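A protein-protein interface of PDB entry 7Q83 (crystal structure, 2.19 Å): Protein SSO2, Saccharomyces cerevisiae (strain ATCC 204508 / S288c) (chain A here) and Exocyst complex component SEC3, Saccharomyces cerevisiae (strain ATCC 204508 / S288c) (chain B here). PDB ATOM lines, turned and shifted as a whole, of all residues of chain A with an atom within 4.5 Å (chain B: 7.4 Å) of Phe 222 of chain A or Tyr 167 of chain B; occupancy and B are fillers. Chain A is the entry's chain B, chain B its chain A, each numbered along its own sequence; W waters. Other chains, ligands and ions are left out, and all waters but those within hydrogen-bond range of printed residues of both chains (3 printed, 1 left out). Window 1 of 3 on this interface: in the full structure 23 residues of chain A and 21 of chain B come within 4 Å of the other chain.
Gln 128 of chain A touches Tyr 167 of chain B (OE1 to CE1, 3.3 Å). Leu 131 of chain A touches Tyr 167 of chain B. Tyr 167 of chain B touches Lys 132 of chain A. Tyr 167 of chain B touches Gln 135 of chain A. Gln 135 of chain A touches Leu 168 of chain B (CG to CD2, 3.7 Å). Arg 138 of chain A touches Ile 148 of chain B. NH2 of Arg 138 of chain A touches CB of Gln 149 of chain B, at 3.8 Å. Gln 149 of chain B touches Thr 219 of chain A (CG to CG2, 3.6 Å). Phe 222 of chain A touches Tyr 167 of chain B (CZ to CD2, 3.2 Å). Asn 223 of chain A touches Gln 149 of chain B.
NZ of Lys 141 of chain B lies within hydrogen-bond range of OH of Tyr 167 of chain B (2.7 Å). O of Leu 163 of chain B is in hydrogen-bond range of N of Leu 168 of chain B (3.1 Å). OD1 of Asp 169 of chain B lies within hydrogen-bond range of N of Ser 172 of chain B (2.9 Å). The guanidinium group (NH2) of Arg 138 of chain A sits at hydrogen-bond distance from the side-chain hydroxyl (OG1) of Thr 219 of chain A, at 3.1 Å.
Water W1 bridges OD1 of Asp 169 of chain B and NZ of Lys 132 of chain A. Water W2 lies within hydrogen-bond range of OG of Ser 172 of chain B, O of Tyr 167 of chain B and O of Lys 132 of chain A. Water W3 lies within hydrogen-bond range of the side-chain amide nitrogen (NE2) of Gln 128 of chain A and the backbone carbonyl oxygen (O) of Ser 164 of chain B.
OH of Tyr 167 of chain B sits at hydrogen-bond distance from OE2 of Glu 226 of chain A, at 2.8 Å. The side-chain amino group of Lys 132 of chain A lies within salt-bridge range of the side-chain carboxylate of Asp 169 of chain B (2.9 Å). The backbone carbonyl oxygen (O) of Phe 166 of chain B lies within hydrogen-bond range of the side-chain amide nitrogen (NE2) of Gln 135 of chain A (3.2 Å).
Of the 15 printed residues of chain A, 9 touch a printed residue of chain B. Of the 14 printed residues of chain B, 6 touch a printed residue of chain A. Hydrophobic or aromatic side chains of chain B that line the printed part of chain A: Ile 148, Tyr 167 and Leu 168.
Printed residues of chain B within 4 Å of Gln 128 of chain A: Tyr 167. Printed residues of chain B within 4 Å of Lys 132 of chain A: Tyr 167 (3.6 Å) and Asp 169 (2.9 Å). Phe 222 of chain A touches just one residue of chain B: Tyr 167. Printed residues of chain A within 4 Å of Ile 148 of chain B: Gln 135 and Arg 138. Ser 164 of chain B touches none of the printed residues of chain A. Leu 165 of chain B touches none of the printed residues of chain A. Of the printed residues of chain A, Phe 166 of chain B touches Gln 135 (3.2 Å). Tyr 167 of chain B touches just these residues of chain A: Gln 128 (3.3 Å), Leu 131 (3.5 Å), Lys 132 (3.6 Å), Gln 135 (3.4 Å), Phe 222 (3.2 Å) and Glu 226 (2.8 Å). Of the printed residues of chain A, Asp 169 of chain B touches Lys 132 (2.9 Å). The nearest residue of chain B that does not touch Phe 222 of chain A is Thr 145 of chain B (4.3 Å). The nearest printed residue of chain A that does not touch Leu 168 of chain B is Lys 132 of chain A (4.6 Å).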
ATOM      1  N   GLN A 128      12.009 -31.817   6.720  1.00  0.00           N
ATOM      2  CA  GLN A 128      13.434 -32.128   6.643  1.00  0.00           C
ATOM      3  C   GLN A 128      13.993 -31.825   5.257  1.00  0.00           C
ATOM      4  O   GLN A 128      15.088 -31.264   5.136  1.00  0.00           O
ATOM      5  CB  GLN A 128      13.676 -33.594   7.004  1.00  0.00           C
ATOM      6  CG  GLN A 128      13.131 -34.002   8.364  1.00  0.00           C
ATOM      7  CD  GLN A 128      14.167 -33.892   9.462  1.00  0.00           C
ATOM      8  OE1 GLN A 128      14.369 -32.820  10.034  1.00  0.00           O
ATOM      9  NE2 GLN A 128      14.829 -35.003   9.764  1.00  0.00           N
ATOM     10  N   LEU A 131      14.496 -28.044   5.074  1.00  0.00           N
ATOM     11  CA  LEU A 131      15.635 -27.547   5.842  1.00  0.00           C
ATOM     12  C   LEU A 131      16.957 -27.862   5.152  1.00  0.00           C
ATOM     13  O   LEU A 131      17.888 -27.049   5.178  1.00  0.00           O
ATOM     14  CB  LEU A 131      15.606 -28.136   7.252  1.00  0.00           C
ATOM     15  CG  LEU A 131      14.463 -27.585   8.106  1.00  0.00           C
ATOM     16  CD1 LEU A 131      14.356 -28.319   9.429  1.00  0.00           C
ATOM     17  CD2 LEU A 131      14.650 -26.094   8.330  1.00  0.00           C
ATOM     18  N   LYS A 132      17.061 -29.038   4.528  1.00  0.00           N
ATOM     19  CA  LYS A 132      18.286 -29.387   3.818  1.00  0.00           C
ATOM     20  C   LYS A 132      18.511 -28.461   2.630  1.00  0.00           C
ATOM     21  O   LYS A 132      19.644 -28.044   2.363  1.00  0.00           O
ATOM     22  CB  LYS A 132      18.232 -30.847   3.367  1.00  0.00           C
ATOM     23  CG  LYS A 132      19.552 -31.393   2.849  1.00  0.00           C
ATOM     24  CD  LYS A 132      19.597 -31.392   1.328  1.00  0.00           C
ATOM     25  CE  LYS A 132      20.970 -31.789   0.814  1.00  0.00           C
ATOM     26  NZ  LYS A 132      21.082 -31.609  -0.657  1.00  0.00           N
ATOM     27  N   ILE A 134      17.309 -25.345   2.318  1.00  0.00           N
ATOM     28  CA  ILE A 134      17.676 -24.049   2.885  1.00  0.00           C
ATOM     29  C   ILE A 134      19.145 -24.049   3.283  1.00  0.00           C
ATOM     30  O   ILE A 134      19.859 -23.056   3.093  1.00  0.00           O
ATOM     31  CB  ILE A 134      16.762 -23.707   4.077  1.00  0.00           C
ATOM     32  CG1 ILE A 134      15.319 -23.506   3.610  1.00  0.00           C
ATOM     33  CG2 ILE A 134      17.261 -22.465   4.801  1.00  0.00           C
ATOM     34  CD1 ILE A 134      14.283 -23.904   4.643  1.00  0.00           C
ATOM     35  N   GLN A 135      19.620 -25.167   3.839  1.00  0.00           N
ATOM     36  CA  GLN A 135      21.037 -25.299   4.156  1.00  0.00           C
ATOM     37  C   GLN A 135      21.885 -25.319   2.891  1.00  0.00           C
ATOM     38  O   GLN A 135      22.987 -24.759   2.866  1.00  0.00           O
ATOM     39  CB  GLN A 135      21.270 -26.562   4.985  1.00  0.00           C
ATOM     40  CG  GLN A 135      22.559 -26.551   5.790  1.00  0.00           C
ATOM     41  CD  GLN A 135      22.434 -25.767   7.082  1.00  0.00           C
ATOM     42  OE1 GLN A 135      22.253 -24.549   7.066  1.00  0.00           O
ATOM     43  NE2 GLN A 135      22.530 -26.463   8.210  1.00  0.00           N
ATOM     44  N   ARG A 138      22.109 -21.694   1.802  1.00  0.00           N
ATOM     45  CA  ARG A 138      22.977 -20.915   2.682  1.00  0.00           C
ATOM     46  C   ARG A 138      24.450 -21.174   2.386  1.00  0.00           C
ATOM     47  O   ARG A 138      25.262 -20.241   2.384  1.00  0.00           O
ATOM     48  CB  ARG A 138      22.651 -21.239   4.139  1.00  0.00           C
ATOM     49  CG  ARG A 138      23.615 -20.653   5.152  1.00  0.00           C
ATOM     50  CD  ARG A 138      23.524 -21.391   6.474  1.00  0.00           C
ATOM     51  NE  ARG A 138      22.649 -20.711   7.421  1.00  0.00           N
ATOM     52  CZ  ARG A 138      21.839 -21.328   8.273  1.00  0.00           C
ATOM     53  NH1 ARG A 138      21.759 -22.647   8.320  1.00  0.00           N
ATOM     54  NH2 ARG A 138      21.095 -20.600   9.101  1.00  0.00           N
ATOM     55  N   LEU A 218      17.502 -16.487   5.422  1.00  0.00           N
ATOM     56  CA  LEU A 218      17.610 -17.940   5.493  1.00  0.00           C
ATOM     57  C   LEU A 218      17.785 -18.403   6.933  1.00  0.00           C
ATOM     58  O   LEU A 218      17.256 -19.449   7.326  1.00  0.00           O
ATOM     59  CB  LEU A 218      18.768 -18.427   4.623  1.00  0.00           C
ATOM     60  CG  LEU A 218      18.674 -18.136   3.122  1.00  0.00           C
ATOM     61  CD1 LEU A 218      19.898 -18.677   2.395  1.00  0.00           C
ATOM     62  CD2 LEU A 218      17.399 -18.722   2.536  1.00  0.00           C
ATOM     63  N   THR A 219      18.516 -17.628   7.737  1.00  0.00           N
ATOM     64  CA  THR A 219      18.629 -17.929   9.161  1.00  0.00           C
ATOM     65  C   THR A 219      17.289 -17.750   9.865  1.00  0.00           C
ATOM     66  O   THR A 219      16.866 -18.609  10.647  1.00  0.00           O
ATOM     67  CB  THR A 219      19.698 -17.039   9.799  1.00  0.00           C
ATOM     68  OG1 THR A 219      20.997 -17.488   9.399  1.00  0.00           O
ATOM     69  CG2 THR A 219      19.597 -17.081  11.315  1.00  0.00           C
ATOM     70  N   GLN A 220      16.603 -16.635   9.594  1.00  0.00           N
ATOM     71  CA  GLN A 220      15.281 -16.416  10.170  1.00  0.00           C
ATOM     72  C   GLN A 220      14.296 -17.485   9.712  1.00  0.00           C
ATOM     73  O   GLN A 220      13.478 -17.968  10.505  1.00  0.00           O
ATOM     74  CB  GLN A 220      14.773 -15.023   9.796  1.00  0.00           C
ATOM     75  CG  GLN A 220      13.466 -14.636  10.464  1.00  0.00           C
ATOM     76  CD  GLN A 220      13.586 -14.572  11.973  1.00  0.00           C
ATOM     77  OE1 GLN A 220      14.343 -13.766  12.514  1.00  0.00           O
ATOM     78  NE2 GLN A 220      12.840 -15.428  12.661  1.00  0.00           N
ATOM     79  N   LEU A 221      14.361 -17.866   8.434  1.00  0.00           N
ATOM     80  CA  LEU A 221      13.495 -18.926   7.928  1.00  0.00           C
ATOM     81  C   LEU A 221      13.862 -20.272   8.539  1.00  0.00           C
ATOM     82  O   LEU A 221      12.981 -21.084   8.845  1.00  0.00           O
ATOM     83  CB  LEU A 221      13.582 -18.986   6.405  1.00  0.00           C
ATOM     84  CG  LEU A 221      13.116 -20.283   5.746  1.00  0.00           C
ATOM     85  CD1 LEU A 221      11.596 -20.389   5.776  1.00  0.00           C
ATOM     86  CD2 LEU A 221      13.631 -20.346   4.326  1.00  0.00           C
ATOM     87  N   PHE A 222      15.161 -20.523   8.713  1.00  0.00           N
ATOM     88  CA  PHE A 222      15.613 -21.738   9.380  1.00  0.00           C
ATOM     89  C   PHE A 222      14.990 -21.870  10.764  1.00  0.00           C
ATOM     90  O   PHE A 222      14.573 -22.962  11.167  1.00  0.00           O
ATOM     91  CB  PHE A 222      17.136 -21.727   9.486  1.00  0.00           C
ATOM     92  CG  PHE A 222      17.766 -23.080   9.408  1.00  0.00           C
ATOM     93  CD1 PHE A 222      17.954 -23.701   8.186  1.00  0.00           C
ATOM     94  CD2 PHE A 222      18.200 -23.721  10.558  1.00  0.00           C
ATOM     95  CE1 PHE A 222      18.547 -24.945   8.111  1.00  0.00           C
ATOM     96  CE2 PHE A 222      18.794 -24.965  10.489  1.00  0.00           C
ATOM     97  CZ  PHE A 222      18.969 -25.574   9.262  1.00  0.00           C
ATOM     98  N   ASN A 223      14.915 -20.763  11.504  1.00  0.00           N
ATOM     99  CA  ASN A 223      14.388 -20.809  12.862  1.00  0.00           C
ATOM    100  C   ASN A 223      12.871 -20.951  12.871  1.00  0.00           C
ATOM    101  O   ASN A 223      12.319 -21.638  13.737  1.00  0.00           O
ATOM    102  CB  ASN A 223      14.814 -19.559  13.625  1.00  0.00           C
ATOM    103  CG  ASN A 223      16.249 -19.634  14.099  1.00  0.00           C
ATOM    104  OD1 ASN A 223      16.839 -20.714  14.163  1.00  0.00           O
ATOM    105  ND2 ASN A 223      16.824 -18.484  14.431  1.00  0.00           N
ATOM    106  N   ASP A 224      12.185 -20.302  11.927  1.00  0.00           N
ATOM    107  CA  ASP A 224      10.736 -20.451  11.840  1.00  0.00           C
ATOM    108  C   ASP A 224      10.347 -21.906  11.616  1.00  0.00           C
ATOM    109  O   ASP A 224       9.363 -22.391  12.186  1.00  0.00           O
ATOM    110  CB  ASP A 224      10.180 -19.574  10.716  1.00  0.00           C
ATOM    111  CG  ASP A 224      10.273 -18.093  11.025  1.00  0.00           C
ATOM    112  OD1 ASP A 224      10.518 -17.738  12.198  1.00  0.00           O
ATOM    113  OD2 ASP A 224      10.100 -17.282  10.090  1.00  0.00           O
ATOM    114  N   MET A 225      11.117 -22.623  10.798  1.00  0.00           N
ATOM    115  CA  MET A 225      10.790 -24.010  10.491  1.00  0.00           C
ATOM    116  C   MET A 225      11.065 -24.944  11.662  1.00  0.00           C
ATOM    117  O   MET A 225      10.494 -26.039  11.710  1.00  0.00           O
ATOM    118  CB  MET A 225      11.569 -24.468   9.259  1.00  0.00           C
ATOM    119  CG  MET A 225      11.080 -23.870   7.947  1.00  0.00           C
ATOM    120  SD  MET A 225       9.285 -23.696   7.861  1.00  0.00           S
ATOM    121  CE  MET A 225       8.788 -25.417   7.802  1.00  0.00           C
ATOM    122  N   GLU A 226      11.922 -24.544  12.601  1.00  0.00           N
ATOM    123  CA  GLU A 226      12.179 -25.353  13.783  1.00  0.00           C
ATOM    124  C   GLU A 226      11.180 -25.097  14.899  1.00  0.00           C
ATOM    125  O   GLU A 226      11.069 -25.922  15.813  1.00  0.00           O
ATOM    126  CB  GLU A 226      13.601 -25.105  14.297  1.00  0.00           C
ATOM    127  CG  GLU A 226      14.695 -25.362  13.265  1.00  0.00           C
ATOM    128  CD  GLU A 226      15.097 -26.825  13.173  1.00  0.00           C
ATOM    129  OE1 GLU A 226      14.230 -27.704  13.366  1.00  0.00           O
ATOM    130  OE2 GLU A 226      16.287 -27.095  12.906  1.00  0.00           O
ATOM    131  N   LYS B 141      23.546 -31.780  17.717  1.00  0.00           N
ATOM    132  CA  LYS B 141      22.691 -31.126  16.733  1.00  0.00           C
ATOM    133  C   LYS B 141      22.577 -29.633  17.016  1.00  0.00           C
ATOM    134  O   LYS B 141      22.794 -28.804  16.126  1.00  0.00           O
ATOM    135  CB  LYS B 141      21.311 -31.784  16.734  1.00  0.00           C
ATOM    136  CG  LYS B 141      20.343 -31.234  15.705  1.00  0.00           C
ATOM    137  CD  LYS B 141      19.083 -32.083  15.649  1.00  0.00           C
ATOM    138  CE  LYS B 141      17.925 -31.315  15.046  1.00  0.00           C
ATOM    139  NZ  LYS B 141      18.061 -31.221  13.572  1.00  0.00           N
ATOM    140  N   THR B 145      24.254 -26.965  14.484  1.00  0.00           N
ATOM    141  CA  THR B 145      23.280 -26.036  13.919  1.00  0.00           C
ATOM    142  C   THR B 145      23.616 -24.597  14.291  1.00  0.00           C
ATOM    143  O   THR B 145      23.545 -23.696  13.446  1.00  0.00           O
ATOM    144  CB  THR B 145      21.874 -26.400  14.399  1.00  0.00           C
ATOM    145  OG1 THR B 145      21.403 -27.540  13.668  1.00  0.00           O
ATOM    146  CG2 THR B 145      20.910 -25.240  14.199  1.00  0.00           C
ATOM    147  N   LEU B 146      23.993 -24.364  15.551  1.00  0.00           N
ATOM    148  CA  LEU B 146      24.398 -23.026  15.968  1.00  0.00           C
ATOM    149  C   LEU B 146      25.619 -22.551  15.188  1.00  0.00           C
ATOM    150  O   LEU B 146      25.665 -21.401  14.735  1.00  0.00           O
ATOM    151  CB  LEU B 146      24.685 -23.013  17.470  1.00  0.00           C
ATOM    152  CG  LEU B 146      24.847 -21.659  18.165  1.00  0.00           C
ATOM    153  CD1 LEU B 146      23.831 -20.645  17.653  1.00  0.00           C
ATOM    154  CD2 LEU B 146      24.733 -21.829  19.671  1.00  0.00           C
ATOM    155  N   ILE B 148      26.751 -23.526  12.153  1.00  0.00           N
ATOM    156  CA  ILE B 148      26.457 -23.276  10.745  1.00  0.00           C
ATOM    157  C   ILE B 148      25.712 -21.958  10.585  1.00  0.00           C
ATOM    158  O   ILE B 148      25.969 -21.192   9.648  1.00  0.00           O
ATOM    159  CB  ILE B 148      25.673 -24.461  10.150  1.00  0.00           C
ATOM    160  CG1 ILE B 148      26.546 -25.718  10.145  1.00  0.00           C
ATOM    161  CG2 ILE B 148      25.195 -24.140   8.742  1.00  0.00           C
ATOM    162  CD1 ILE B 148      25.808 -26.976   9.755  1.00  0.00           C
ATOM    163  N   GLN B 149      24.795 -21.664  11.510  1.00  0.00           N
ATOM    164  CA  GLN B 149      24.078 -20.395  11.469  1.00  0.00           C
ATOM    165  C   GLN B 149      24.992 -19.230  11.836  1.00  0.00           C
ATOM    166  O   GLN B 149      24.947 -18.172  11.196  1.00  0.00           O
ATOM    167  CB  GLN B 149      22.873 -20.442  12.408  1.00  0.00           C
ATOM    168  CG  GLN B 149      22.292 -19.073  12.729  1.00  0.00           C
ATOM    169  CD  GLN B 149      21.358 -19.090  13.922  1.00  0.00           C
ATOM    170  OE1 GLN B 149      20.500 -19.963  14.037  1.00  0.00           O
ATOM    171  NE2 GLN B 149      21.511 -18.113  14.810  1.00  0.00           N
ATOM    172  N   ASP B 162      25.929 -38.852  11.257  1.00  0.00           N
ATOM    173  CA  ASP B 162      24.969 -38.793  10.161  1.00  0.00           C
ATOM    174  C   ASP B 162      24.764 -37.330   9.787  1.00  0.00           C
ATOM    175  O   ASP B 162      24.239 -36.546  10.585  1.00  0.00           O
ATOM    176  CB  ASP B 162      23.655 -39.453  10.578  1.00  0.00           C
ATOM    177  CG  ASP B 162      22.648 -39.560   9.435  1.00  0.00           C
ATOM    178  OD1 ASP B 162      22.703 -38.756   8.477  1.00  0.00           O
ATOM    179  OD2 ASP B 162      21.784 -40.460   9.504  1.00  0.00           O
ATOM    180  N   LEU B 163      25.186 -36.957   8.576  1.00  0.00           N
ATOM    181  CA  LEU B 163      25.108 -35.560   8.157  1.00  0.00           C
ATOM    182  C   LEU B 163      23.669 -35.060   8.104  1.00  0.00           C
ATOM    183  O   LEU B 163      23.424 -33.863   8.300  1.00  0.00           O
ATOM    184  CB  LEU B 163      25.779 -35.382   6.793  1.00  0.00           C
ATOM    185  CG  LEU B 163      27.297 -35.572   6.734  1.00  0.00           C
ATOM    186  CD1 LEU B 163      27.759 -35.690   5.290  1.00  0.00           C
ATOM    187  CD2 LEU B 163      28.022 -34.437   7.438  1.00  0.00           C
ATOM    188  N   SER B 164      22.707 -35.951   7.841  1.00  0.00           N
ATOM    189  CA  SER B 164      21.309 -35.536   7.771  1.00  0.00           C
ATOM    190  C   SER B 164      20.821 -34.961   9.093  1.00  0.00           C
ATOM    191  O   SER B 164      19.875 -34.166   9.108  1.00  0.00           O
ATOM    192  CB  SER B 164      20.429 -36.715   7.363  1.00  0.00           C
ATOM    193  OG  SER B 164      20.463 -37.733   8.347  1.00  0.00           O
ATOM    194  N   LEU B 165      21.445 -35.354  10.209  1.00  0.00           N
ATOM    195  CA  LEU B 165      21.099 -34.775  11.504  1.00  0.00           C
ATOM    196  C   LEU B 165      21.235 -33.258  11.494  1.00  0.00           C
ATOM    197  O   LEU B 165      20.467 -32.558  12.166  1.00  0.00           O
ATOM    198  CB  LEU B 165      21.983 -35.381  12.592  1.00  0.00           C
ATOM    199  CG  LEU B 165      21.670 -35.008  14.039  1.00  0.00           C
ATOM    200  CD1 LEU B 165      20.290 -35.513  14.433  1.00  0.00           C
ATOM    201  CD2 LEU B 165      22.744 -35.555  14.973  1.00  0.00           C
ATOM    202  N   PHE B 166      22.197 -32.736  10.737  1.00  0.00           N
ATOM    203  CA  PHE B 166      22.437 -31.305  10.624  1.00  0.00           C
ATOM    204  C   PHE B 166      21.886 -30.722   9.330  1.00  0.00           C
ATOM    205  O   PHE B 166      22.241 -29.594   8.971  1.00  0.00           O
ATOM    206  CB  PHE B 166      23.935 -31.023  10.736  1.00  0.00           C
ATOM    207  CG  PHE B 166      24.619 -31.841  11.787  1.00  0.00           C
ATOM    208  CD1 PHE B 166      24.292 -31.684  13.123  1.00  0.00           C
ATOM    209  CD2 PHE B 166      25.575 -32.780  11.439  1.00  0.00           C
ATOM    210  CE1 PHE B 166      24.916 -32.440  14.097  1.00  0.00           C
ATOM    211  CE2 PHE B 166      26.203 -33.539  12.405  1.00  0.00           C
ATOM    212  CZ  PHE B 166      25.874 -33.370  13.738  1.00  0.00           C
ATOM    213  N   TYR B 167      21.031 -31.469   8.629  1.00  0.00           N
ATOM    214  CA  TYR B 167      20.463 -31.053   7.345  1.00  0.00           C
ATOM    215  C   TYR B 167      21.557 -30.834   6.302  1.00  0.00           C
ATOM    216  O   TYR B 167      21.513 -29.889   5.512  1.00  0.00           O
ATOM    217  CB  TYR B 167      19.587 -29.808   7.496  1.00  0.00           C
ATOM    218  CG  TYR B 167      18.694 -29.825   8.717  1.00  0.00           C
ATOM    219  CD1 TYR B 167      17.866 -30.906   8.992  1.00  0.00           C
ATOM    220  CD2 TYR B 167      18.680 -28.754   9.595  1.00  0.00           C
ATOM    221  CE1 TYR B 167      17.047 -30.912  10.114  1.00  0.00           C
ATOM    222  CE2 TYR B 167      17.867 -28.747  10.711  1.00  0.00           C
ATOM    223  CZ  TYR B 167      17.055 -29.827  10.969  1.00  0.00           C
ATOM    224  OH  TYR B 167      16.252 -29.809  12.087  1.00  0.00           O
ATOM    225  N   LEU B 168      22.547 -31.720   6.301  1.00  0.00           N
ATOM    226  CA  LEU B 168      23.594 -31.743   5.296  1.00  0.00           C
ATOM    227  C   LEU B 168      23.574 -33.081   4.570  1.00  0.00           C
ATOM    228  O   LEU B 168      23.029 -34.072   5.062  1.00  0.00           O
ATOM    229  CB  LEU B 168      24.981 -31.525   5.917  1.00  0.00           C
ATOM    230  CG  LEU B 168      25.218 -30.308   6.812  1.00  0.00           C
ATOM    231  CD1 LEU B 168      26.499 -30.491   7.621  1.00  0.00           C
ATOM    232  CD2 LEU B 168      25.280 -29.033   5.985  1.00  0.00           C
ATOM    233  N   ASP B 169      24.169 -33.097   3.384  1.00  0.00           N
ATOM    234  CA  ASP B 169      24.546 -34.339   2.724  1.00  0.00           C
ATOM    235  C   ASP B 169      26.043 -34.281   2.435  1.00  0.00           C
ATOM    236  O   ASP B 169      26.744 -33.365   2.881  1.00  0.00           O
ATOM    237  CB  ASP B 169      23.696 -34.604   1.473  1.00  0.00           C
ATOM    238  CG  ASP B 169      23.877 -33.550   0.385  1.00  0.00           C
ATOM    239  OD1 ASP B 169      24.705 -32.631   0.536  1.00  0.00           O
ATOM    240  OD2 ASP B 169      23.171 -33.654  -0.643  1.00  0.00           O
ATOM    241  N   SER B 172      27.221 -31.130   0.314  1.00  0.00           N
ATOM    242  CA  SER B 172      26.998 -29.887   1.047  1.00  0.00           C
ATOM    243  C   SER B 172      27.966 -29.763   2.218  1.00  0.00           C
ATOM    244  O   SER B 172      28.371 -28.651   2.574  1.00  0.00           O
ATOM    245  CB  SER B 172      25.548 -29.790   1.533  1.00  0.00           C
ATOM    246  OG  SER B 172      25.372 -30.374   2.813  1.00  0.00           O
HETATM  247  O   HOH W   1      23.897 -30.630  -1.070  1.00  0.00           O
HETATM  248  O   HOH W   2      22.855 -28.798   3.077  1.00  0.00           O
HETATM  249  O   HOH W   3      17.443 -33.989  11.017  1.00  0.00           O
